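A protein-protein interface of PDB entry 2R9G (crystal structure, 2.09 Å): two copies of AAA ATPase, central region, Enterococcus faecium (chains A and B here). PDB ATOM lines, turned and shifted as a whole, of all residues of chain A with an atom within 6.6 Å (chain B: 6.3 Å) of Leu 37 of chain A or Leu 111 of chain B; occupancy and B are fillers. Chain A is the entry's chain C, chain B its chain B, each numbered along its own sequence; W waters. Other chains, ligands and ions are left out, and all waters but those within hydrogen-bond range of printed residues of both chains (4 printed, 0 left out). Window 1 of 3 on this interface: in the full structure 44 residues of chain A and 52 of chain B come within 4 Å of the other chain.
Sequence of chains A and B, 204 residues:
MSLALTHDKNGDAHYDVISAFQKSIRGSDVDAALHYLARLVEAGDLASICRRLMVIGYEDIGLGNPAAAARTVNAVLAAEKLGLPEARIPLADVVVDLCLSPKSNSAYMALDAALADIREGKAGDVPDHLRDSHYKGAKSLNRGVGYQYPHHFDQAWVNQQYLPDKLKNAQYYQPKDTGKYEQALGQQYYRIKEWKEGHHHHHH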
ATOM      1  N   VAL A  17      16.390  -6.342  -2.984  1.00  0.00           N
ATOM      2  CA  VAL A  17      15.866  -7.374  -3.884  1.00  0.00           C
ATOM      3  C   VAL A  17      16.695  -8.644  -3.698  1.00  0.00           C
ATOM      4  O   VAL A  17      16.144  -9.738  -3.605  1.00  0.00           O
ATOM      5  CB  VAL A  17      15.853  -6.922  -5.376  1.00  0.00           C
ATOM      6  CG1 VAL A  17      15.203  -7.972  -6.255  1.00  0.00           C
ATOM      7  CG2 VAL A  17      15.098  -5.613  -5.532  1.00  0.00           C
ATOM      8  N   PHE A  21      15.310 -12.151  -2.326  1.00  0.00           N
ATOM      9  CA  PHE A  21      15.630 -13.330  -3.131  1.00  0.00           C
ATOM     10  C   PHE A  21      16.202 -14.478  -2.282  1.00  0.00           C
ATOM     11  O   PHE A  21      15.684 -15.589  -2.335  1.00  0.00           O
ATOM     12  CB  PHE A  21      16.598 -12.913  -4.260  1.00  0.00           C
ATOM     13  CG  PHE A  21      17.017 -14.032  -5.196  1.00  0.00           C
ATOM     14  CD1 PHE A  21      16.077 -14.802  -5.867  1.00  0.00           C
ATOM     15  CD2 PHE A  21      18.366 -14.257  -5.454  1.00  0.00           C
ATOM     16  CE1 PHE A  21      16.474 -15.801  -6.747  1.00  0.00           C
ATOM     17  CE2 PHE A  21      18.775 -15.256  -6.335  1.00  0.00           C
ATOM     18  CZ  PHE A  21      17.824 -16.033  -6.979  1.00  0.00           C
ATOM     19  N   ALA A  32       7.684 -16.454  -4.869  1.00  0.00           N
ATOM     20  CA  ALA A  32       8.338 -15.235  -4.417  1.00  0.00           C
ATOM     21  C   ALA A  32       9.777 -15.191  -4.894  1.00  0.00           C
ATOM     22  O   ALA A  32      10.255 -14.144  -5.315  1.00  0.00           O
ATOM     23  CB  ALA A  32       8.272 -15.119  -2.916  1.00  0.00           C
ATOM     24  N   ALA A  33      10.459 -16.333  -4.854  1.00  0.00           N
ATOM     25  CA  ALA A  33      11.847 -16.413  -5.324  1.00  0.00           C
ATOM     26  C   ALA A  33      11.956 -16.164  -6.818  1.00  0.00           C
ATOM     27  O   ALA A  33      12.909 -15.528  -7.279  1.00  0.00           O
ATOM     28  CB  ALA A  33      12.457 -17.743  -4.964  1.00  0.00           C
ATOM     29  N   LEU A  34      10.974 -16.649  -7.568  1.00  0.00           N
ATOM     30  CA  LEU A  34      10.930 -16.435  -9.008  1.00  0.00           C
ATOM     31  C   LEU A  34      10.575 -14.996  -9.345  1.00  0.00           C
ATOM     32  O   LEU A  34      11.072 -14.449 -10.327  1.00  0.00           O
ATOM     33  CB  LEU A  34       9.978 -17.421  -9.683  1.00  0.00           C
ATOM     34  CG  LEU A  34      10.504 -18.864  -9.782  1.00  0.00           C
ATOM     35  CD1 LEU A  34       9.485 -19.722 -10.480  1.00  0.00           C
ATOM     36  CD2 LEU A  34      11.848 -18.958 -10.504  1.00  0.00           C
ATOM     37  N   HIS A  35       9.740 -14.382  -8.507  1.00  0.00           N
ATOM     38  CA  HIS A  35       9.436 -12.965  -8.628  1.00  0.00           C
ATOM     39  C   HIS A  35      10.688 -12.113  -8.451  1.00  0.00           C
ATOM     40  O   HIS A  35      10.950 -11.224  -9.265  1.00  0.00           O
ATOM     41  CB  HIS A  35       8.373 -12.541  -7.614  1.00  0.00           C
ATOM     42  CG  HIS A  35       8.338 -11.065  -7.377  1.00  0.00           C
ATOM     43  ND1 HIS A  35       7.862 -10.177  -8.316  1.00  0.00           N
ATOM     44  CD2 HIS A  35       8.754 -10.319  -6.329  1.00  0.00           C
ATOM     45  CE1 HIS A  35       7.971  -8.947  -7.849  1.00  0.00           C
ATOM     46  NE2 HIS A  35       8.511  -9.005  -6.646  1.00  0.00           N
ATOM     47  N   TYR A  36      11.459 -12.390  -7.398  1.00  0.00           N
ATOM     48  CA  TYR A  36      12.691 -11.641  -7.139  1.00  0.00           C
ATOM     49  C   TYR A  36      13.802 -11.951  -8.125  1.00  0.00           C
ATOM     50  O   TYR A  36      14.582 -11.057  -8.455  1.00  0.00           O
ATOM     51  CB  TYR A  36      13.167 -11.789  -5.689  1.00  0.00           C
ATOM     52  CG  TYR A  36      12.195 -11.163  -4.717  1.00  0.00           C
ATOM     53  CD1 TYR A  36      11.937  -9.788  -4.742  1.00  0.00           C
ATOM     54  CD2 TYR A  36      11.504 -11.947  -3.803  1.00  0.00           C
ATOM     55  CE1 TYR A  36      11.017  -9.212  -3.859  1.00  0.00           C
ATOM     56  CE2 TYR A  36      10.586 -11.393  -2.931  1.00  0.00           C
ATOM     57  CZ  TYR A  36      10.351 -10.031  -2.956  1.00  0.00           C
ATOM     58  OH  TYR A  36       9.450  -9.504  -2.069  1.00  0.00           O
ATOM     59  N   LEU A  37      13.862 -13.194  -8.611  1.00  0.00           N
ATOM     60  CA  LEU A  37      14.798 -13.533  -9.689  1.00  0.00           C
ATOM     61  C   LEU A  37      14.482 -12.701 -10.932  1.00  0.00           C
ATOM     62  O   LEU A  37      15.389 -12.118 -11.537  1.00  0.00           O
ATOM     63  CB  LEU A  37      14.812 -15.036 -10.009  1.00  0.00           C
ATOM     64  CG  LEU A  37      15.601 -15.515 -11.243  1.00  0.00           C
ATOM     65  CD1 LEU A  37      17.067 -15.057 -11.228  1.00  0.00           C
ATOM     66  CD2 LEU A  37      15.517 -17.019 -11.397  1.00  0.00           C
ATOM     67  N   ALA A  38      13.192 -12.624 -11.263  1.00  0.00           N
ATOM     68  CA  ALA A  38      12.699 -11.859 -12.401  1.00  0.00           C
ATOM     69  C   ALA A  38      13.099 -10.385 -12.348  1.00  0.00           C
ATOM     70  O   ALA A  38      13.503  -9.820 -13.356  1.00  0.00           O
ATOM     71  CB  ALA A  38      11.204 -12.003 -12.512  1.00  0.00           C
ATOM     72  N   ARG A  39      12.989  -9.784 -11.166  1.00  0.00           N
ATOM     73  CA  ARG A  39      13.388  -8.402 -10.934  1.00  0.00           C
ATOM     74  C   ARG A  39      14.884  -8.208 -11.120  1.00  0.00           C
ATOM     75  O   ARG A  39      15.318  -7.186 -11.647  1.00  0.00           O
ATOM     76  CB  ARG A  39      13.001  -7.967  -9.522  1.00  0.00           C
ATOM     77  CG  ARG A  39      11.529  -7.719  -9.359  1.00  0.00           C
ATOM     78  CD  ARG A  39      11.168  -7.457  -7.934  1.00  0.00           C
ATOM     79  NE  ARG A  39      11.414  -6.079  -7.524  1.00  0.00           N
ATOM     80  CZ  ARG A  39      10.806  -5.494  -6.497  1.00  0.00           C
ATOM     81  NH1 ARG A  39       9.894  -6.158  -5.784  1.00  0.00           N
ATOM     82  NH2 ARG A  39      11.100  -4.238  -6.191  1.00  0.00           N
ATOM     83  N   LEU A  40      15.657  -9.191 -10.672  1.00  0.00           N
ATOM     84  CA  LEU A  40      17.104  -9.179 -10.820  1.00  0.00           C
ATOM     85  C   LEU A  40      17.540  -9.364 -12.270  1.00  0.00           C
ATOM     86  O   LEU A  40      18.456  -8.685 -12.729  1.00  0.00           O
ATOM     87  CB  LEU A  40      17.739 -10.243  -9.923  1.00  0.00           C
ATOM     88  CG  LEU A  40      17.676  -9.968  -8.420  1.00  0.00           C
ATOM     89  CD1 LEU A  40      18.102 -11.208  -7.673  1.00  0.00           C
ATOM     90  CD2 LEU A  40      18.519  -8.740  -8.009  1.00  0.00           C
ATOM     91  N   VAL A  41      16.867 -10.272 -12.973  1.00  0.00           N
ATOM     92  CA  VAL A  41      17.081 -10.499 -14.402  1.00  0.00           C
ATOM     93  C   VAL A  41      16.801  -9.211 -15.189  1.00  0.00           C
ATOM     94  O   VAL A  41      17.611  -8.805 -16.016  1.00  0.00           O
ATOM     95  CB  VAL A  41      16.228 -11.696 -14.937  1.00  0.00           C
ATOM     96  CG1 VAL A  41      16.108 -11.679 -16.467  1.00  0.00           C
ATOM     97  CG2 VAL A  41      16.814 -13.023 -14.474  1.00  0.00           C
ATOM     98  N   GLU A  42      15.678  -8.563 -14.886  1.00  0.00           N
ATOM     99  CA  GLU A  42      15.326  -7.274 -15.483  1.00  0.00           C
ATOM    100  C   GLU A  42      16.376  -6.185 -15.240  1.00  0.00           C
ATOM    101  O   GLU A  42      16.655  -5.396 -16.134  1.00  0.00           O
ATOM    102  CB  GLU A  42      13.952  -6.804 -15.001  1.00  0.00           C
ATOM    103  CG  GLU A  42      12.788  -7.482 -15.695  1.00  0.00           C
ATOM    104  CD  GLU A  42      12.786  -7.255 -17.197  1.00  0.00           C
ATOM    105  OE1 GLU A  42      12.435  -6.138 -17.632  1.00  0.00           O
ATOM    106  OE2 GLU A  42      13.130  -8.198 -17.942  1.00  0.00           O
ATOM    107  N   ILE A  49      23.579 -12.150  -9.674  1.00  0.00           N
ATOM    108  CA  ILE A  49      22.582 -13.219  -9.513  1.00  0.00           C
ATOM    109  C   ILE A  49      23.287 -14.564  -9.284  1.00  0.00           C
ATOM    110  O   ILE A  49      22.941 -15.311  -8.365  1.00  0.00           O
ATOM    111  CB  ILE A  49      21.629 -13.352 -10.741  1.00  0.00           C
ATOM    112  CG1 ILE A  49      20.873 -12.047 -11.010  1.00  0.00           C
ATOM    113  CG2 ILE A  49      20.627 -14.488 -10.512  1.00  0.00           C
ATOM    114  CD1 ILE A  49      20.195 -11.965 -12.392  1.00  0.00           C
ATOM    115  N   LEU A  53      23.170 -16.852  -5.984  1.00  0.00           N
ATOM    116  CA  LEU A  53      22.609 -18.203  -6.107  1.00  0.00           C
ATOM    117  C   LEU A  53      23.519 -19.299  -5.541  1.00  0.00           C
ATOM    118  O   LEU A  53      23.032 -20.208  -4.881  1.00  0.00           O
ATOM    119  CB  LEU A  53      22.214 -18.519  -7.552  1.00  0.00           C
ATOM    120  CG  LEU A  53      20.965 -19.390  -7.728  1.00  0.00           C
ATOM    121  CD1 LEU A  53      19.957 -19.165  -6.611  1.00  0.00           C
ATOM    122  CD2 LEU A  53      20.323 -19.070  -9.043  1.00  0.00           C
ATOM    123  N   ARG A  88      18.703 -16.971 -17.906  1.00  0.00           N
ATOM    124  CA  ARG A  88      17.592 -17.027 -16.955  1.00  0.00           C
ATOM    125  C   ARG A  88      17.001 -18.431 -16.793  1.00  0.00           C
ATOM    126  O   ARG A  88      16.365 -18.727 -15.773  1.00  0.00           O
ATOM    127  CB  ARG A  88      16.488 -16.043 -17.376  1.00  0.00           C
ATOM    128  CG  ARG A  88      15.430 -16.628 -18.332  1.00  0.00           C
ATOM    129  CD  ARG A  88      14.608 -15.554 -19.030  1.00  0.00           C
ATOM    130  NE  ARG A  88      13.605 -16.134 -19.931  1.00  0.00           N
ATOM    131  CZ  ARG A  88      13.844 -16.551 -21.176  1.00  0.00           C
ATOM    132  NH1 ARG A  88      12.857 -17.057 -21.899  1.00  0.00           N
ATOM    133  NH2 ARG A  88      15.062 -16.476 -21.704  1.00  0.00           N
ATOM    134  N   ILE A  89      17.207 -19.282 -17.801  1.00  0.00           N
ATOM    135  CA  ILE A  89      16.603 -20.612 -17.839  1.00  0.00           C
ATOM    136  C   ILE A  89      17.260 -21.595 -16.848  1.00  0.00           C
ATOM    137  O   ILE A  89      16.555 -22.118 -15.984  1.00  0.00           O
ATOM    138  CB  ILE A  89      16.516 -21.175 -19.285  1.00  0.00           C
ATOM    139  CG1 ILE A  89      15.714 -20.235 -20.189  1.00  0.00           C
ATOM    140  CG2 ILE A  89      15.913 -22.554 -19.266  1.00  0.00           C
ATOM    141  CD1 ILE A  89      15.898 -20.503 -21.692  1.00  0.00           C
ATOM    142  N   LEU A  91      19.007 -20.740 -14.304  1.00  0.00           N
ATOM    143  CA  LEU A  91      18.804 -20.107 -12.991  1.00  0.00           C
ATOM    144  C   LEU A  91      17.424 -20.387 -12.421  1.00  0.00           C
ATOM    145  O   LEU A  91      17.301 -20.626 -11.226  1.00  0.00           O
ATOM    146  CB  LEU A  91      19.033 -18.600 -13.053  1.00  0.00           C
ATOM    147  CG  LEU A  91      20.442 -18.190 -13.478  1.00  0.00           C
ATOM    148  CD1 LEU A  91      20.537 -16.688 -13.535  1.00  0.00           C
ATOM    149  CD2 LEU A  91      21.509 -18.802 -12.545  1.00  0.00           C
ATOM    150  N   ALA A  92      16.400 -20.347 -13.274  1.00  0.00           N
ATOM    151  CA  ALA A  92      15.031 -20.703 -12.872  1.00  0.00           C
ATOM    152  C   ALA A  92      14.955 -22.134 -12.365  1.00  0.00           C
ATOM    153  O   ALA A  92      14.345 -22.398 -11.309  1.00  0.00           O
ATOM    154  CB  ALA A  92      14.052 -20.507 -14.029  1.00  0.00           C
ATOM    155  N   ASP A  93      15.578 -23.048 -13.118  1.00  0.00           N
ATOM    156  CA  ASP A  93      15.626 -24.455 -12.769  1.00  0.00           C
ATOM    157  C   ASP A  93      16.206 -24.677 -11.381  1.00  0.00           C
ATOM    158  O   ASP A  93      15.656 -25.449 -10.595  1.00  0.00           O
ATOM    159  CB  ASP A  93      16.471 -25.235 -13.781  1.00  0.00           C
ATOM    160  CG  ASP A  93      15.771 -25.448 -15.112  1.00  0.00           C
ATOM    161  OD1 ASP A  93      16.445 -25.979 -16.010  1.00  0.00           O
ATOM    162  OD2 ASP A  93      14.580 -25.097 -15.274  1.00  0.00           O
ATOM    163  N   VAL A  95      16.614 -22.418  -8.934  1.00  0.00           N
ATOM    164  CA  VAL A  95      15.845 -21.700  -7.918  1.00  0.00           C
ATOM    165  C   VAL A  95      14.688 -22.568  -7.406  1.00  0.00           C
ATOM    166  O   VAL A  95      14.525 -22.737  -6.198  1.00  0.00           O
ATOM    167  CB  VAL A  95      15.372 -20.305  -8.434  1.00  0.00           C
ATOM    168  CG1 VAL A  95      14.223 -19.749  -7.607  1.00  0.00           C
ATOM    169  CG2 VAL A  95      16.525 -19.316  -8.425  1.00  0.00           C
ATOM    170  N   SER B 106       8.471 -26.576 -16.559  1.00  0.00           N
ATOM    171  CA  SER B 106       7.742 -25.871 -15.502  1.00  0.00           C
ATOM    172  C   SER B 106       8.455 -24.641 -14.932  1.00  0.00           C
ATOM    173  O   SER B 106       7.836 -23.590 -14.783  1.00  0.00           O
ATOM    174  CB  SER B 106       7.364 -26.835 -14.376  1.00  0.00           C
ATOM    175  OG  SER B 106       8.525 -27.366 -13.768  1.00  0.00           O
ATOM    176  N   ALA B 107       9.749 -24.777 -14.639  1.00  0.00           N
ATOM    177  CA  ALA B 107      10.534 -23.690 -14.050  1.00  0.00           C
ATOM    178  C   ALA B 107      10.780 -22.549 -15.039  1.00  0.00           C
ATOM    179  O   ALA B 107      10.777 -21.381 -14.656  1.00  0.00           O
ATOM    180  CB  ALA B 107      11.855 -24.222 -13.513  1.00  0.00           C
ATOM    181  N   TYR B 108      11.003 -22.916 -16.300  1.00  0.00           N
ATOM    182  CA  TYR B 108      11.158 -21.982 -17.409  1.00  0.00           C
ATOM    183  C   TYR B 108       9.892 -21.135 -17.564  1.00  0.00           C
ATOM    184  O   TYR B 108       9.962 -19.900 -17.623  1.00  0.00           O
ATOM    185  CB  TYR B 108      11.479 -22.778 -18.686  1.00  0.00           C
ATOM    186  CG  TYR B 108      11.318 -22.056 -20.012  1.00  0.00           C
ATOM    187  CD1 TYR B 108      12.122 -20.965 -20.343  1.00  0.00           C
ATOM    188  CD2 TYR B 108      10.390 -22.502 -20.957  1.00  0.00           C
ATOM    189  CE1 TYR B 108      11.988 -20.314 -21.576  1.00  0.00           C
ATOM    190  CE2 TYR B 108      10.247 -21.861 -22.192  1.00  0.00           C
ATOM    191  CZ  TYR B 108      11.052 -20.768 -22.493  1.00  0.00           C
ATOM    192  OH  TYR B 108      10.919 -20.134 -23.710  1.00  0.00           O
ATOM    193  N   MET B 109       8.750 -21.825 -17.598  1.00  0.00           N
ATOM    194  CA  MET B 109       7.467 -21.156 -17.732  1.00  0.00           C
ATOM    195  C   MET B 109       7.094 -20.308 -16.519  1.00  0.00           C
ATOM    196  O   MET B 109       6.500 -19.244 -16.682  1.00  0.00           O
ATOM    197  CB  MET B 109       6.371 -22.163 -18.087  1.00  0.00           C
ATOM    198  CG  MET B 109       6.619 -22.865 -19.425  1.00  0.00           C
ATOM    199  SD  MET B 109       5.952 -22.059 -20.896  1.00  0.00           S
ATOM    200  CE  MET B 109       7.003 -20.652 -21.156  1.00  0.00           C
ATOM    201  N   ALA B 110       7.470 -20.760 -15.324  1.00  0.00           N
ATOM    202  CA  ALA B 110       7.171 -20.049 -14.091  1.00  0.00           C
ATOM    203  C   ALA B 110       7.913 -18.713 -14.003  1.00  0.00           C
ATOM    204  O   ALA B 110       7.336 -17.709 -13.603  1.00  0.00           O
ATOM    205  CB  ALA B 110       7.490 -20.919 -12.910  1.00  0.00           C
ATOM    206  N   LEU B 111       9.183 -18.700 -14.394  1.00  0.00           N
ATOM    207  CA  LEU B 111       9.949 -17.464 -14.373  1.00  0.00           C
ATOM    208  C   LEU B 111       9.445 -16.467 -15.422  1.00  0.00           C
ATOM    209  O   LEU B 111       9.354 -15.265 -15.152  1.00  0.00           O
ATOM    210  CB  LEU B 111      11.452 -17.729 -14.530  1.00  0.00           C
ATOM    211  CG  LEU B 111      12.275 -16.432 -14.490  1.00  0.00           C
ATOM    212  CD1 LEU B 111      12.184 -15.731 -13.104  1.00  0.00           C
ATOM    213  CD2 LEU B 111      13.700 -16.672 -14.906  1.00  0.00           C
ATOM    214  N   ASP B 112       9.091 -16.962 -16.603  1.00  0.00           N
ATOM    215  CA  ASP B 112       8.550 -16.085 -17.641  1.00  0.00           C
ATOM    216  C   ASP B 112       7.163 -15.507 -17.307  1.00  0.00           C
ATOM    217  O   ASP B 112       6.824 -14.412 -17.759  1.00  0.00           O
ATOM    218  CB  ASP B 112       8.587 -16.759 -19.011  1.00  0.00           C
ATOM    219  CG  ASP B 112       9.989 -16.790 -19.604  1.00  0.00           C
ATOM    220  OD1 ASP B 112      10.949 -16.306 -18.950  1.00  0.00           O
ATOM    221  OD2 ASP B 112      10.137 -17.302 -20.729  1.00  0.00           O
ATOM    222  N   ALA B 113       6.386 -16.223 -16.494  1.00  0.00           N
ATOM    223  CA  ALA B 113       5.145 -15.672 -15.952  1.00  0.00           C
ATOM    224  C   ALA B 113       5.444 -14.590 -14.908  1.00  0.00           C
ATOM    225  O   ALA B 113       4.714 -13.597 -14.810  1.00  0.00           O
ATOM    226  CB  ALA B 113       4.270 -16.779 -15.357  1.00  0.00           C
ATOM    227  N   ALA B 114       6.512 -14.791 -14.133  1.00  0.00           N
ATOM    228  CA  ALA B 114       6.966 -13.794 -13.159  1.00  0.00           C
ATOM    229  C   ALA B 114       7.457 -12.520 -13.841  1.00  0.00           C
ATOM    230  O   ALA B 114       7.144 -11.414 -13.387  1.00  0.00           O
ATOM    231  CB  ALA B 114       8.047 -14.366 -12.242  1.00  0.00           C
ATOM    232  N   LEU B 115       8.230 -12.697 -14.915  1.00  0.00           N
ATOM    233  CA  LEU B 115       8.758 -11.598 -15.725  1.00  0.00           C
ATOM    234  C   LEU B 115       7.651 -10.789 -16.407  1.00  0.00           C
ATOM    235  O   LEU B 115       7.727  -9.558 -16.464  1.00  0.00           O
ATOM    236  CB  LEU B 115       9.739 -12.126 -16.777  1.00  0.00           C
ATOM    237  CG  LEU B 115      11.137 -12.443 -16.270  1.00  0.00           C
ATOM    238  CD1 LEU B 115      11.848 -13.422 -17.193  1.00  0.00           C
ATOM    239  CD2 LEU B 115      11.928 -11.149 -16.109  1.00  0.00           C
ATOM    240  N   ALA B 116       6.628 -11.487 -16.906  1.00  0.00           N
ATOM    241  CA  ALA B 116       5.449 -10.852 -17.493  1.00  0.00           C
ATOM    242  C   ALA B 116       4.735  -9.937 -16.496  1.00  0.00           C
ATOM    243  O   ALA B 116       4.340  -8.833 -16.860  1.00  0.00           O
ATOM    244  CB  ALA B 116       4.500 -11.891 -18.044  1.00  0.00           C
ATOM    245  N   TYR B 172       3.066 -18.715  -9.987  1.00  0.00           N
ATOM    246  CA  TYR B 172       3.821 -18.882 -11.218  1.00  0.00           C
ATOM    247  C   TYR B 172       4.148 -20.344 -11.489  1.00  0.00           C
ATOM    248  O   TYR B 172       4.065 -20.799 -12.624  1.00  0.00           O
ATOM    249  CB  TYR B 172       5.114 -18.061 -11.156  1.00  0.00           C
ATOM    250  CG  TYR B 172       4.899 -16.599 -10.852  1.00  0.00           C
ATOM    251  CD1 TYR B 172       4.101 -15.807 -11.675  1.00  0.00           C
ATOM    252  CD2 TYR B 172       5.497 -16.007  -9.747  1.00  0.00           C
ATOM    253  CE1 TYR B 172       3.896 -14.467 -11.400  1.00  0.00           C
ATOM    254  CE2 TYR B 172       5.309 -14.664  -9.467  1.00  0.00           C
ATOM    255  CZ  TYR B 172       4.506 -13.902 -10.297  1.00  0.00           C
ATOM    256  OH  TYR B 172       4.320 -12.576 -10.025  1.00  0.00           O
HETATM  257  O   HOH W   1      12.216 -18.506 -17.913  1.00  0.00           O
HETATM  258  O   HOH W   2       6.480 -11.295 -10.807  1.00  0.00           O
HETATM  259  O   HOH W   3      12.526 -25.748 -17.269  1.00  0.00           O
HETATM  260  O   HOH W   4      13.236 -18.836 -24.271  1.00  0.00           O
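The side-chain carboxylate (OD1) of Asp 112 of chain B lies within salt-bridge range of the guanidinium group (NE) of Arg 88 of chain A (2.8 Å).
Among the printed residues, pairs that only touch across the chains: Leu 34 of chain A with Ala 110 of chain B, Leu 34 of chain A with Leu 111 of chain B, Leu 34 of chain A with Ala 114 of chain B, Leu 37 of chain A with Leu 111 of chain B, Ala 38 of chain A with Leu 111 of chain B, Ala 38 of chain A with Ala 114 of chain B, Ala 38 of chain A with Leu 115 of chain B, Glu 42 of chain A with Leu 115 of chain B, Arg 88 of chain A with Tyr 108 of chain B, Arg 88 of chain A with Leu 111 of chain B, Arg 88 of chain A with Leu 115 of chain B, Ile 89 of chain A with Tyr 108 of chain B, Ala 92 of chain A with Ala 107 of chain B, Ala 92 of chain A with Leu 111 of chain B and Asp 93 of chain A with Ala 107 of chain B.
Printed residues of chain B within 4 Å of Leu 37 of chain A: Leu 111 (3.9 Å).
Printed residues of chain B within 4 Å of Arg 88 of chain A: Tyr 108, Leu 111, Asp 112 and Leu 115.
Printed residues of chain A within 4 Å of Ala 107 of chain B: Ala 92 (3.4 Å) and Asp 93 (3.4 Å).
Of the printed residues of chain A, Tyr 108 of chain B touches Arg 88 (3.4 Å) and Ile 89 (3.7 Å).
Met 109 of chain B touches none of the printed residues of chain A.
Of the printed residues of chain A, Asp 112 of chain B touches Arg 88 (2.8 Å).
Of the printed residues of chain A, Ala 114 of chain B touches Leu 34 and Ala 38.
The nearest residue of chain B that does not touch Leu 37 of chain A is Leu 115 of chain B (5.8 Å).
The nearest printed residue of chain A that does not touch Leu 115 of chain B is Val 41 of chain A (4.2 Å).
Of the 12 printed residues of chain B, 7 touch a printed residue of chain A.
Printed residues of chain B that touch a printed residue of chain A: Ala 107, Tyr 108, Ala 110, Leu 111, Asp 112, Ala 114 and Leu 115.
Hydrophobic or aromatic side chains of chain B that line the printed part of chain A: Ala 107, Tyr 108, Ala 110, Leu 111, Ala 114 and Leu 115.
Hydrophobic or aromatic side chains of chain A within 4 Å of the printed part of chain B: Leu 34, Leu 37, Ala 38, Ile 89 and Ala 92.
Among the printed residues, Asp or Glu carboxylates within 4 Å of a Lys or Arg side-chain nitrogen of the other chain: Arg 88 of chain A with Asp 112 of chain B (2.8 Å).
No position is printed for both chains.
Water W2 lies within hydrogen-bond range of the side-chain hydroxyl (OH) of Tyr 172 of chain B (2.6 Å), the backbone carbonyl oxygen (O) of Ala 114 of chain B (2.7 Å) and a ring nitrogen (ND1) of His 35 of chain A (3.1 Å).
Water W1 lies within hydrogen-bond range of O of Tyr 108 of chain B (2.7 Å), OD1 of Asp 112 of chain B (2.7 Å) and NE of Arg 88 of chain A (3.4 Å).
Water W4 bridges OH of Tyr 108 of chain B and NH1 of Arg 88 of chain A.
Water W3 bridges the side-chain carboxylate (OD2) of Asp 93 of chain A (2.9 Å) and the backbone NH (N) of Tyr 108 of chain B (3.4 Å).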
